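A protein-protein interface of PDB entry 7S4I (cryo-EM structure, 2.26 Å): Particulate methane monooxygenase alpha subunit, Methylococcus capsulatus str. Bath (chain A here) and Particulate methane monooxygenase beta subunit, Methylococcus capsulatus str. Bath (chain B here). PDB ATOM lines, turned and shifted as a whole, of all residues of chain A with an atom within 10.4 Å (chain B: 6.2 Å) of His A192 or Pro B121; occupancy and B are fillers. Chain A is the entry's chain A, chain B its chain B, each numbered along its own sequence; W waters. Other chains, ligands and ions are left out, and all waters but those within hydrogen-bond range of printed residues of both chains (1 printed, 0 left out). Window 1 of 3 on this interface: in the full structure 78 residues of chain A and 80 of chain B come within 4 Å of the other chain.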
ATOM      1  N   ASN A 184     -29.132  -1.529   2.351  1.00  0.00           N
ATOM      2  CA  ASN A 184     -28.225  -2.521   2.927  1.00  0.00           C
ATOM      3  C   ASN A 184     -27.262  -1.930   3.953  1.00  0.00           C
ATOM      4  O   ASN A 184     -26.447  -2.675   4.517  1.00  0.00           O
ATOM      5  CB  ASN A 184     -27.420  -3.264   1.849  1.00  0.00           C
ATOM      6  CG  ASN A 184     -26.853  -4.575   2.342  1.00  0.00           C
ATOM      7  OD1 ASN A 184     -27.546  -5.356   2.989  1.00  0.00           O
ATOM      8  ND2 ASN A 184     -25.587  -4.825   2.036  1.00  0.00           N
ATOM      9  N   GLU A 185     -27.331  -0.626   4.224  1.00  0.00           N
ATOM     10  CA  GLU A 185     -26.414  -0.010   5.179  1.00  0.00           C
ATOM     11  C   GLU A 185     -26.612  -0.576   6.579  1.00  0.00           C
ATOM     12  O   GLU A 185     -25.641  -0.885   7.282  1.00  0.00           O
ATOM     13  CB  GLU A 185     -26.610   1.505   5.179  1.00  0.00           C
ATOM     14  CG  GLU A 185     -25.469   2.290   5.792  1.00  0.00           C
ATOM     15  CD  GLU A 185     -25.799   3.761   5.945  1.00  0.00           C
ATOM     16  OE1 GLU A 185     -26.167   4.398   4.936  1.00  0.00           O
ATOM     17  OE2 GLU A 185     -25.694   4.282   7.075  1.00  0.00           O
ATOM     18  N   GLY A 186     -27.870  -0.714   7.002  1.00  0.00           N
ATOM     19  CA  GLY A 186     -28.140  -1.268   8.319  1.00  0.00           C
ATOM     20  C   GLY A 186     -27.654  -2.697   8.456  1.00  0.00           C
ATOM     21  O   GLY A 186     -27.068  -3.070   9.472  1.00  0.00           O
ATOM     22  N   ASN A 187     -27.891  -3.515   7.429  1.00  0.00           N
ATOM     23  CA  ASN A 187     -27.441  -4.902   7.461  1.00  0.00           C
ATOM     24  C   ASN A 187     -25.919  -4.988   7.523  1.00  0.00           C
ATOM     25  O   ASN A 187     -25.361  -5.786   8.289  1.00  0.00           O
ATOM     26  CB  ASN A 187     -27.979  -5.642   6.236  1.00  0.00           C
ATOM     27  CG  ASN A 187     -27.505  -7.074   6.161  1.00  0.00           C
ATOM     28  OD1 ASN A 187     -27.822  -7.889   7.025  1.00  0.00           O
ATOM     29  ND2 ASN A 187     -26.747  -7.394   5.119  1.00  0.00           N
ATOM     30  N   THR A 188     -25.233  -4.167   6.722  1.00  0.00           N
ATOM     31  CA  THR A 188     -23.774  -4.151   6.747  1.00  0.00           C
ATOM     32  C   THR A 188     -23.250  -3.756   8.122  1.00  0.00           C
ATOM     33  O   THR A 188     -22.370  -4.431   8.679  1.00  0.00           O
ATOM     34  CB  THR A 188     -23.241  -3.190   5.685  1.00  0.00           C
ATOM     35  OG1 THR A 188     -23.688  -3.606   4.390  1.00  0.00           O
ATOM     36  CG2 THR A 188     -21.728  -3.164   5.711  1.00  0.00           C
ATOM     37  N   TYR A 189     -23.788  -2.671   8.685  1.00  0.00           N
ATOM     38  CA  TYR A 189     -23.376  -2.234  10.013  1.00  0.00           C
ATOM     39  C   TYR A 189     -23.621  -3.322  11.046  1.00  0.00           C
ATOM     40  O   TYR A 189     -22.759  -3.599  11.887  1.00  0.00           O
ATOM     41  CB  TYR A 189     -24.120  -0.957  10.401  1.00  0.00           C
ATOM     42  CG  TYR A 189     -23.489   0.314   9.893  1.00  0.00           C
ATOM     43  CD1 TYR A 189     -22.110   0.439   9.800  1.00  0.00           C
ATOM     44  CD2 TYR A 189     -24.272   1.396   9.516  1.00  0.00           C
ATOM     45  CE1 TYR A 189     -21.531   1.602   9.340  1.00  0.00           C
ATOM     46  CE2 TYR A 189     -23.702   2.562   9.056  1.00  0.00           C
ATOM     47  CZ  TYR A 189     -22.332   2.660   8.970  1.00  0.00           C
ATOM     48  OH  TYR A 189     -21.760   3.823   8.513  1.00  0.00           O
ATOM     49  N   PHE A 190     -24.793  -3.958  10.991  1.00  0.00           N
ATOM     50  CA  PHE A 190     -25.139  -4.978  11.971  1.00  0.00           C
ATOM     51  C   PHE A 190     -24.162  -6.142  11.922  1.00  0.00           C
ATOM     52  O   PHE A 190     -23.645  -6.580  12.954  1.00  0.00           O
ATOM     53  CB  PHE A 190     -26.568  -5.472  11.736  1.00  0.00           C
ATOM     54  CG  PHE A 190     -26.881  -6.760  12.441  1.00  0.00           C
ATOM     55  CD1 PHE A 190     -27.240  -6.761  13.777  1.00  0.00           C
ATOM     56  CD2 PHE A 190     -26.810  -7.971  11.770  1.00  0.00           C
ATOM     57  CE1 PHE A 190     -27.524  -7.942  14.431  1.00  0.00           C
ATOM     58  CE2 PHE A 190     -27.091  -9.155  12.420  1.00  0.00           C
ATOM     59  CZ  PHE A 190     -27.450  -9.141  13.752  1.00  0.00           C
ATOM     60  N   TRP A 191     -23.906  -6.670  10.724  1.00  0.00           N
ATOM     61  CA  TRP A 191     -23.040  -7.841  10.628  1.00  0.00           C
ATOM     62  C   TRP A 191     -21.608  -7.507  11.025  1.00  0.00           C
ATOM     63  O   TRP A 191     -20.953  -8.288  11.736  1.00  0.00           O
ATOM     64  CB  TRP A 191     -23.099  -8.424   9.219  1.00  0.00           C
ATOM     65  CG  TRP A 191     -24.286  -9.306   9.029  1.00  0.00           C
ATOM     66  CD1 TRP A 191     -25.322  -9.112   8.167  1.00  0.00           C
ATOM     67  CD2 TRP A 191     -24.579 -10.511   9.745  1.00  0.00           C
ATOM     68  NE1 TRP A 191     -26.236 -10.128   8.290  1.00  0.00           N
ATOM     69  CE2 TRP A 191     -25.802 -11.001   9.251  1.00  0.00           C
ATOM     70  CE3 TRP A 191     -23.921 -11.228  10.748  1.00  0.00           C
ATOM     71  CZ2 TRP A 191     -26.382 -12.172   9.727  1.00  0.00           C
ATOM     72  CZ3 TRP A 191     -24.498 -12.390  11.218  1.00  0.00           C
ATOM     73  CH2 TRP A 191     -25.716 -12.850  10.710  1.00  0.00           C
ATOM     74  N   HIS A 192     -21.104  -6.348  10.591  1.00  0.00           N
ATOM     75  CA  HIS A 192     -19.744  -5.976  10.963  1.00  0.00           C
ATOM     76  C   HIS A 192     -19.619  -5.776  12.468  1.00  0.00           C
ATOM     77  O   HIS A 192     -18.652  -6.243  13.081  1.00  0.00           O
ATOM     78  CB  HIS A 192     -19.313  -4.724  10.204  1.00  0.00           C
ATOM     79  CG  HIS A 192     -18.623  -5.021   8.911  1.00  0.00           C
ATOM     80  ND1 HIS A 192     -17.294  -5.382   8.844  1.00  0.00           N
ATOM     81  CD2 HIS A 192     -19.078  -5.028   7.636  1.00  0.00           C
ATOM     82  CE1 HIS A 192     -16.960  -5.591   7.583  1.00  0.00           C
ATOM     83  NE2 HIS A 192     -18.025  -5.383   6.831  1.00  0.00           N
ATOM     84  N   ALA A 193     -20.598  -5.106  13.084  1.00  0.00           N
ATOM     85  CA  ALA A 193     -20.573  -4.918  14.530  1.00  0.00           C
ATOM     86  C   ALA A 193     -20.671  -6.249  15.262  1.00  0.00           C
ATOM     87  O   ALA A 193     -20.004  -6.448  16.280  1.00  0.00           O
ATOM     88  CB  ALA A 193     -21.705  -3.985  14.957  1.00  0.00           C
ATOM     89  N   PHE A 194     -21.493  -7.172  14.759  1.00  0.00           N
ATOM     90  CA  PHE A 194     -21.636  -8.477  15.396  1.00  0.00           C
ATOM     91  C   PHE A 194     -20.316  -9.238  15.395  1.00  0.00           C
ATOM     92  O   PHE A 194     -19.888  -9.771  16.427  1.00  0.00           O
ATOM     93  CB  PHE A 194     -22.731  -9.275  14.682  1.00  0.00           C
ATOM     94  CG  PHE A 194     -22.832 -10.708  15.121  1.00  0.00           C
ATOM     95  CD1 PHE A 194     -23.633 -11.060  16.193  1.00  0.00           C
ATOM     96  CD2 PHE A 194     -22.149 -11.707  14.445  1.00  0.00           C
ATOM     97  CE1 PHE A 194     -23.737 -12.378  16.595  1.00  0.00           C
ATOM     98  CE2 PHE A 194     -22.247 -13.025  14.843  1.00  0.00           C
ATOM     99  CZ  PHE A 194     -23.044 -13.360  15.918  1.00  0.00           C
ATOM    100  N   TRP A 195     -19.647  -9.293  14.241  1.00  0.00           N
ATOM    101  CA  TRP A 195     -18.399 -10.049  14.182  1.00  0.00           C
ATOM    102  C   TRP A 195     -17.291  -9.355  14.966  1.00  0.00           C
ATOM    103  O   TRP A 195     -16.481 -10.017  15.632  1.00  0.00           O
ATOM    104  CB  TRP A 195     -17.998 -10.284  12.728  1.00  0.00           C
ATOM    105  CG  TRP A 195     -18.811 -11.371  12.098  1.00  0.00           C
ATOM    106  CD1 TRP A 195     -19.642 -11.255  11.024  1.00  0.00           C
ATOM    107  CD2 TRP A 195     -18.900 -12.735  12.530  1.00  0.00           C
ATOM    108  NE1 TRP A 195     -20.230 -12.465  10.749  1.00  0.00           N
ATOM    109  CE2 TRP A 195     -19.792 -13.390  11.659  1.00  0.00           C
ATOM    110  CE3 TRP A 195     -18.305 -13.468  13.562  1.00  0.00           C
ATOM    111  CZ2 TRP A 195     -20.103 -14.740  11.789  1.00  0.00           C
ATOM    112  CZ3 TRP A 195     -18.617 -14.807  13.690  1.00  0.00           C
ATOM    113  CH2 TRP A 195     -19.507 -15.430  12.808  1.00  0.00           C
ATOM    114  N   PHE A 196     -17.251  -8.020  14.924  1.00  0.00           N
ATOM    115  CA  PHE A 196     -16.290  -7.290  15.740  1.00  0.00           C
ATOM    116  C   PHE A 196     -16.522  -7.554  17.221  1.00  0.00           C
ATOM    117  O   PHE A 196     -15.568  -7.708  17.989  1.00  0.00           O
ATOM    118  CB  PHE A 196     -16.377  -5.796  15.436  1.00  0.00           C
ATOM    119  CG  PHE A 196     -15.117  -5.042  15.736  1.00  0.00           C
ATOM    120  CD1 PHE A 196     -14.877  -4.542  17.004  1.00  0.00           C
ATOM    121  CD2 PHE A 196     -14.170  -4.830  14.748  1.00  0.00           C
ATOM    122  CE1 PHE A 196     -13.718  -3.847  17.282  1.00  0.00           C
ATOM    123  CE2 PHE A 196     -13.008  -4.137  15.020  1.00  0.00           C
ATOM    124  CZ  PHE A 196     -12.782  -3.645  16.290  1.00  0.00           C
ATOM    125  N   ALA A 197     -17.790  -7.612  17.638  1.00  0.00           N
ATOM    126  CA  ALA A 197     -18.111  -7.907  19.029  1.00  0.00           C
ATOM    127  C   ALA A 197     -17.677  -9.315  19.408  1.00  0.00           C
ATOM    128  O   ALA A 197     -17.199  -9.540  20.521  1.00  0.00           O
ATOM    129  CB  ALA A 197     -19.607  -7.720  19.274  1.00  0.00           C
ATOM    130  N   ILE A 198     -17.851 -10.279  18.501  1.00  0.00           N
ATOM    131  CA  ILE A 198     -17.396 -11.642  18.781  1.00  0.00           C
ATOM    132  C   ILE A 198     -15.887 -11.668  19.003  1.00  0.00           C
ATOM    133  O   ILE A 198     -15.390 -12.266  19.970  1.00  0.00           O
ATOM    134  CB  ILE A 198     -17.817 -12.591  17.641  1.00  0.00           C
ATOM    135  CG1 ILE A 198     -19.313 -12.901  17.722  1.00  0.00           C
ATOM    136  CG2 ILE A 198     -17.006 -13.875  17.685  1.00  0.00           C
ATOM    137  CD1 ILE A 198     -19.738 -13.531  19.026  1.00  0.00           C
ATOM    138  N   GLY A 199     -15.135 -11.010  18.117  1.00  0.00           N
ATOM    139  CA  GLY A 199     -13.688 -10.969  18.282  1.00  0.00           C
ATOM    140  C   GLY A 199     -13.262 -10.265  19.559  1.00  0.00           C
ATOM    141  O   GLY A 199     -12.357 -10.724  20.266  1.00  0.00           O
ATOM    142  N   VAL A 200     -13.913  -9.142  19.871  1.00  0.00           N
ATOM    143  CA  VAL A 200     -13.602  -8.406  21.092  1.00  0.00           C
ATOM    144  C   VAL A 200     -13.929  -9.245  22.319  1.00  0.00           C
ATOM    145  O   VAL A 200     -13.216  -9.197  23.324  1.00  0.00           O
ATOM    146  CB  VAL A 200     -14.347  -7.056  21.101  1.00  0.00           C
ATOM    147  CG1 VAL A 200     -14.342  -6.441  22.491  1.00  0.00           C
ATOM    148  CG2 VAL A 200     -13.718  -6.103  20.098  1.00  0.00           C
ATOM    149  N   ASP B  49     -11.409  -4.620  -1.443  1.00  0.00           N
ATOM    150  CA  ASP B  49     -12.015  -4.238  -0.175  1.00  0.00           C
ATOM    151  C   ASP B  49     -12.699  -2.879  -0.227  1.00  0.00           C
ATOM    152  O   ASP B  49     -13.574  -2.614   0.604  1.00  0.00           O
ATOM    153  CB  ASP B  49     -10.958  -4.236   0.930  1.00  0.00           C
ATOM    154  CG  ASP B  49     -11.568  -4.204   2.316  1.00  0.00           C
ATOM    155  OD1 ASP B  49     -12.310  -5.146   2.661  1.00  0.00           O
ATOM    156  OD2 ASP B  49     -11.311  -3.232   3.056  1.00  0.00           O
ATOM    157  N   PHE B  50     -12.335  -2.022  -1.177  1.00  0.00           N
ATOM    158  CA  PHE B  50     -12.902  -0.683  -1.261  1.00  0.00           C
ATOM    159  C   PHE B  50     -14.316  -0.664  -1.828  1.00  0.00           C
ATOM    160  O   PHE B  50     -15.127   0.170  -1.417  1.00  0.00           O
ATOM    161  CB  PHE B  50     -12.008   0.218  -2.119  1.00  0.00           C
ATOM    162  CG  PHE B  50     -10.731   0.626  -1.450  1.00  0.00           C
ATOM    163  CD1 PHE B  50     -10.555   0.445  -0.089  1.00  0.00           C
ATOM    164  CD2 PHE B  50      -9.699   1.181  -2.187  1.00  0.00           C
ATOM    165  CE1 PHE B  50      -9.376   0.817   0.524  1.00  0.00           C
ATOM    166  CE2 PHE B  50      -8.518   1.554  -1.578  1.00  0.00           C
ATOM    167  CZ  PHE B  50      -8.357   1.371  -0.221  1.00  0.00           C
ATOM    168  N   LYS B  55     -16.326  -6.583  -5.026  1.00  0.00           N
ATOM    169  CA  LYS B  55     -16.499  -7.809  -4.237  1.00  0.00           C
ATOM    170  C   LYS B  55     -17.141  -8.894  -5.103  1.00  0.00           C
ATOM    171  O   LYS B  55     -18.346  -9.152  -5.049  1.00  0.00           O
ATOM    172  CB  LYS B  55     -17.339  -7.543  -2.994  1.00  0.00           C
ATOM    173  CG  LYS B  55     -16.989  -6.273  -2.254  1.00  0.00           C
ATOM    174  CD  LYS B  55     -16.173  -6.555  -1.012  1.00  0.00           C
ATOM    175  CE  LYS B  55     -16.178  -5.367  -0.073  1.00  0.00           C
ATOM    176  NZ  LYS B  55     -15.487  -4.202  -0.678  1.00  0.00           N
ATOM    177  N   LEU B  97      -9.751  -4.338  10.694  1.00  0.00           N
ATOM    178  CA  LEU B  97     -11.131  -3.901  10.527  1.00  0.00           C
ATOM    179  C   LEU B  97     -11.348  -2.518  11.122  1.00  0.00           C
ATOM    180  O   LEU B  97     -12.067  -1.698  10.547  1.00  0.00           O
ATOM    181  CB  LEU B  97     -12.083  -4.914  11.161  1.00  0.00           C
ATOM    182  CG  LEU B  97     -12.397  -6.146  10.313  1.00  0.00           C
ATOM    183  CD1 LEU B  97     -13.011  -7.236  11.166  1.00  0.00           C
ATOM    184  CD2 LEU B  97     -13.320  -5.779   9.167  1.00  0.00           C
ATOM    185  N   GLU B 100      -9.685   0.038   8.775  1.00  0.00           N
ATOM    186  CA  GLU B 100     -10.447   0.118   7.539  1.00  0.00           C
ATOM    187  C   GLU B 100     -11.758   0.861   7.750  1.00  0.00           C
ATOM    188  O   GLU B 100     -12.115   1.733   6.956  1.00  0.00           O
ATOM    189  CB  GLU B 100     -10.700  -1.287   6.993  1.00  0.00           C
ATOM    190  CG  GLU B 100      -9.531  -1.862   6.215  1.00  0.00           C
ATOM    191  CD  GLU B 100      -9.733  -3.315   5.842  1.00  0.00           C
ATOM    192  OE1 GLU B 100     -10.433  -4.029   6.587  1.00  0.00           O
ATOM    193  OE2 GLU B 100      -9.182  -3.746   4.807  1.00  0.00           O
ATOM    194  N   TRP B 101     -12.482   0.542   8.825  1.00  0.00           N
ATOM    195  CA  TRP B 101     -13.759   1.198   9.083  1.00  0.00           C
ATOM    196  C   TRP B 101     -13.581   2.669   9.414  1.00  0.00           C
ATOM    197  O   TRP B 101     -14.384   3.502   8.977  1.00  0.00           O
ATOM    198  CB  TRP B 101     -14.502   0.488  10.214  1.00  0.00           C
ATOM    199  CG  TRP B 101     -15.499  -0.510   9.729  1.00  0.00           C
ATOM    200  CD1 TRP B 101     -15.449  -1.862   9.891  1.00  0.00           C
ATOM    201  CD2 TRP B 101     -16.696  -0.239   8.994  1.00  0.00           C
ATOM    202  NE1 TRP B 101     -16.541  -2.450   9.304  1.00  0.00           N
ATOM    203  CE2 TRP B 101     -17.324  -1.474   8.746  1.00  0.00           C
ATOM    204  CE3 TRP B 101     -17.301   0.930   8.522  1.00  0.00           C
ATOM    205  CZ2 TRP B 101     -18.523  -1.575   8.048  1.00  0.00           C
ATOM    206  CZ3 TRP B 101     -18.490   0.827   7.829  1.00  0.00           C
ATOM    207  CH2 TRP B 101     -19.089  -0.416   7.599  1.00  0.00           C
ATOM    208  N   ARG B 104     -12.997   4.295   6.098  1.00  0.00           N
ATOM    209  CA  ARG B 104     -14.218   4.295   5.298  1.00  0.00           C
ATOM    210  C   ARG B 104     -15.180   5.372   5.773  1.00  0.00           C
ATOM    211  O   ARG B 104     -15.742   6.115   4.961  1.00  0.00           O
ATOM    212  CB  ARG B 104     -14.914   2.934   5.362  1.00  0.00           C
ATOM    213  CG  ARG B 104     -14.159   1.751   4.787  1.00  0.00           C
ATOM    214  CD  ARG B 104     -13.347   2.095   3.565  1.00  0.00           C
ATOM    215  NE  ARG B 104     -12.162   1.253   3.479  1.00  0.00           N
ATOM    216  CZ  ARG B 104     -12.155   0.016   3.002  1.00  0.00           C
ATOM    217  NH1 ARG B 104     -13.258  -0.558   2.551  1.00  0.00           N
ATOM    218  NH2 ARG B 104     -11.013  -0.665   2.983  1.00  0.00           N
ATOM    219  N   ILE B 116     -21.632   4.367   2.610  1.00  0.00           N
ATOM    220  CA  ILE B 116     -21.039   3.274   3.372  1.00  0.00           C
ATOM    221  C   ILE B 116     -21.425   1.929   2.771  1.00  0.00           C
ATOM    222  O   ILE B 116     -20.610   1.000   2.716  1.00  0.00           O
ATOM    223  CB  ILE B 116     -21.449   3.378   4.853  1.00  0.00           C
ATOM    224  CG1 ILE B 116     -20.877   4.657   5.468  1.00  0.00           C
ATOM    225  CG2 ILE B 116     -21.003   2.149   5.629  1.00  0.00           C
ATOM    226  CD1 ILE B 116     -19.435   4.540   5.902  1.00  0.00           C
ATOM    227  N   VAL B 119     -18.818   1.463   0.174  1.00  0.00           N
ATOM    228  CA  VAL B 119     -17.398   1.387   0.507  1.00  0.00           C
ATOM    229  C   VAL B 119     -17.141   0.572   1.777  1.00  0.00           C
ATOM    230  O   VAL B 119     -16.098   0.728   2.404  1.00  0.00           O
ATOM    231  CB  VAL B 119     -16.775   2.788   0.616  1.00  0.00           C
ATOM    232  CG1 VAL B 119     -16.820   3.486  -0.729  1.00  0.00           C
ATOM    233  CG2 VAL B 119     -17.485   3.608   1.680  1.00  0.00           C
ATOM    234  N   PHE B 120     -18.066  -0.302   2.166  1.00  0.00           N
ATOM    235  CA  PHE B 120     -17.854  -1.112   3.357  1.00  0.00           C
ATOM    236  C   PHE B 120     -16.713  -2.110   3.146  1.00  0.00           C
ATOM    237  O   PHE B 120     -16.483  -2.576   2.028  1.00  0.00           O
ATOM    238  CB  PHE B 120     -19.130  -1.864   3.722  1.00  0.00           C
ATOM    239  CG  PHE B 120     -19.589  -2.824   2.666  1.00  0.00           C
ATOM    240  CD1 PHE B 120     -20.423  -2.402   1.647  1.00  0.00           C
ATOM    241  CD2 PHE B 120     -19.189  -4.149   2.692  1.00  0.00           C
ATOM    242  CE1 PHE B 120     -20.842  -3.281   0.672  1.00  0.00           C
ATOM    243  CE2 PHE B 120     -19.607  -5.031   1.720  1.00  0.00           C
ATOM    244  CZ  PHE B 120     -20.435  -4.595   0.709  1.00  0.00           C
ATOM    245  N   PRO B 121     -15.986  -2.452   4.203  1.00  0.00           N
ATOM    246  CA  PRO B 121     -14.941  -3.476   4.105  1.00  0.00           C
ATOM    247  C   PRO B 121     -15.525  -4.879   4.250  1.00  0.00           C
ATOM    248  O   PRO B 121     -16.695  -5.067   4.573  1.00  0.00           O
ATOM    249  CB  PRO B 121     -14.016  -3.135   5.274  1.00  0.00           C
ATOM    250  CG  PRO B 121     -14.919  -2.519   6.279  1.00  0.00           C
ATOM    251  CD  PRO B 121     -15.983  -1.781   5.514  1.00  0.00           C
ATOM    252  N   ALA B 122     -14.676  -5.872   3.998  1.00  0.00           N
ATOM    253  CA  ALA B 122     -15.043  -7.273   4.141  1.00  0.00           C
ATOM    254  C   ALA B 122     -14.929  -7.719   5.593  1.00  0.00           C
ATOM    255  O   ALA B 122     -14.242  -7.095   6.404  1.00  0.00           O
ATOM    256  CB  ALA B 122     -14.161  -8.155   3.258  1.00  0.00           C
ATOM    257  N   SER B 123     -15.618  -8.813   5.915  1.00  0.00           N
ATOM    258  CA  SER B 123     -15.592  -9.393   7.252  1.00  0.00           C
ATOM    259  C   SER B 123     -14.565 -10.519   7.313  1.00  0.00           C
ATOM    260  O   SER B 123     -14.473 -11.332   6.388  1.00  0.00           O
ATOM    261  CB  SER B 123     -16.978  -9.914   7.634  1.00  0.00           C
ATOM    262  OG  SER B 123     -16.986 -10.433   8.951  1.00  0.00           O
ATOM    263  N   LEU B 124     -13.790 -10.562   8.405  1.00  0.00           N
ATOM    264  CA  LEU B 124     -12.696 -11.520   8.553  1.00  0.00           C
ATOM    265  C   LEU B 124     -12.666 -12.186   9.926  1.00  0.00           C
ATOM    266  O   LEU B 124     -11.856 -13.103  10.147  1.00  0.00           O
ATOM    267  CB  LEU B 124     -11.354 -10.834   8.290  1.00  0.00           C
ATOM    268  CG  LEU B 124     -11.296  -9.964   7.036  1.00  0.00           C
ATOM    269  CD1 LEU B 124     -10.395  -8.760   7.256  1.00  0.00           C
ATOM    270  CD2 LEU B 124     -10.861 -10.787   5.839  1.00  0.00           C
ATOM    271  N   VAL B 125     -13.513 -11.738  10.854  1.00  0.00           N
ATOM    272  CA  VAL B 125     -13.498 -12.293  12.208  1.00  0.00           C
ATOM    273  C   VAL B 125     -13.747 -13.798  12.233  1.00  0.00           C
ATOM    274  O   VAL B 125     -13.107 -14.489  13.041  1.00  0.00           O
ATOM    275  CB  VAL B 125     -14.478 -11.518  13.107  1.00  0.00           C
ATOM    276  CG1 VAL B 125     -14.661 -12.238  14.435  1.00  0.00           C
ATOM    277  CG2 VAL B 125     -13.972 -10.108  13.337  1.00  0.00           C
ATOM    278  N   ASN B 160     -19.031 -13.386   4.437  1.00  0.00           N
ATOM    279  CA  ASN B 160     -19.424 -12.103   3.876  1.00  0.00           C
ATOM    280  C   ASN B 160     -20.713 -12.166   3.070  1.00  0.00           C
ATOM    281  O   ASN B 160     -21.229 -11.114   2.680  1.00  0.00           O
ATOM    282  CB  ASN B 160     -18.307 -11.548   2.987  1.00  0.00           C
ATOM    283  CG  ASN B 160     -17.127 -11.042   3.785  1.00  0.00           C
ATOM    284  OD1 ASN B 160     -17.124  -9.905   4.253  1.00  0.00           O
ATOM    285  ND2 ASN B 160     -16.115 -11.883   3.942  1.00  0.00           N
ATOM    286  N   ILE B 163     -23.748  -9.976   4.051  1.00  0.00           N
ATOM    287  CA  ILE B 163     -23.590  -8.547   3.803  1.00  0.00           C
ATOM    288  C   ILE B 163     -23.815  -8.219   2.332  1.00  0.00           C
ATOM    289  O   ILE B 163     -24.531  -7.270   1.997  1.00  0.00           O
ATOM    290  CB  ILE B 163     -22.204  -8.075   4.280  1.00  0.00           C
ATOM    291  CG1 ILE B 163     -22.040  -8.324   5.779  1.00  0.00           C
ATOM    292  CG2 ILE B 163     -22.001  -6.605   3.961  1.00  0.00           C
ATOM    293  CD1 ILE B 163     -20.608  -8.535   6.206  1.00  0.00           C
HETATM  294  O   HOH W   1     -25.028   3.958   2.704  1.00  0.00           O
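Water W1 lies within hydrogen-bond range of the side-chain carboxylate of Glu A185 (2.5 Å) and the backbone NH of Ile B116 (3.4 Å).
Of the printed residues of chain B, His A192 touches Leu B97 (3.97 Å), Trp B101 (3.1 Å), Pro B121 (2.6 Å), Ala B122 (3.3 Å) and Ser B123 (3.9 Å). Of chain A, only His A192 comes within 4 Å of Pro B121. No residue of chain A comes within 4 Å of Glu B100. Of chain A, only Thr A188 comes within 4 Å of Phe B120. Printed residues of chain A within 4 Å of Ala B122: His A192. Printed residues of chain B within 4 Å of Thr A188: Phe B120 (3.5 Å) and Ile B163 (3.5 Å). Printed residues of chain B within 4 Å of Trp A191: Ile B163 (3.6 Å). Printed residues of chain A within 4 Å of Leu B97: His A192 (3.97 Å). Asp B49 touches none of the printed residues of chain A. The nearest residue of chain A that does not touch Pro B121 is Thr A188 (5.5 Å). The nearest printed residue of chain B that does not touch Trp A191 is Ser B123 (5.3 Å).
ND2 of Asn A187 touches CA of Ile B163 (3.6 Å). Phe B120 touches Thr A188. Thr A188 touches Ile B163 (OG1 to CG2, 3.5 Å). Tyr A189 touches Trp B101. Tyr A189 touches Ile B116. Ile B163 touches Trp A191 (CG1 to CB, 3.6 Å). His A192 touches Leu B97 (CE1 to CD2, 3.97 Å). O of Ala B122 touches CE1 of His A192, at 3.3 Å. O of Trp A195 touches CG1 of Val B125, 3.1 Å away. Gly A199 touches Val B125.
Hydrophobic or aromatic side chains of chain A within 4 Å of the printed part of chain B: Tyr A189, Trp A191, His A192 and Trp A195. Hydrophobic or aromatic side chains of chain B within 4 Å of the printed part of chain A: Leu B97, Trp B101, Ile B116, Phe B120, Pro B121, Val B125 and Ile B163. Among the printed residues, 15 pairs touch across the chains. Among the printed residues, no Asp or Glu carboxylate lies within 4 Å of a Lys or Arg side-chain nitrogen of the other chain.
ND2 of Asn A184 lies within hydrogen-bond range of O of Ile B163 (2.7 Å). A ring nitrogen (NE2) of His A192 is in hydrogen-bond range of the backbone carbonyl oxygen (O) of Pro B121, 2.6 Å away. The indole nitrogen of Trp B101 is in hydrogen-bond range of a ring nitrogen (ND1) of His A192 (3.1 Å).
The side-chain amide oxygen (OD1) of Asn A184 lies within hydrogen-bond range of the side-chain amide nitrogen (ND2) of Asn A187 (3.1 Å). N of Ser B123 lies within hydrogen-bond range of OD1 of Asn B160 (2.5 Å). The side-chain amino group (NZ) of Lys B55 sits at hydrogen-bond distance from the backbone carbonyl oxygen (O) of Phe B120 (3.3 Å). OD1 of Asn A187 lies close to NE1 of Trp A191 (3.0 Å). O of Asn A184 sits at hydrogen-bond distance from OG1 of Thr A188. The backbone NH (N) of Ala B122 is in hydrogen-bond range of the side-chain carboxylate (OD1) of Asp B49 (2.8 Å).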
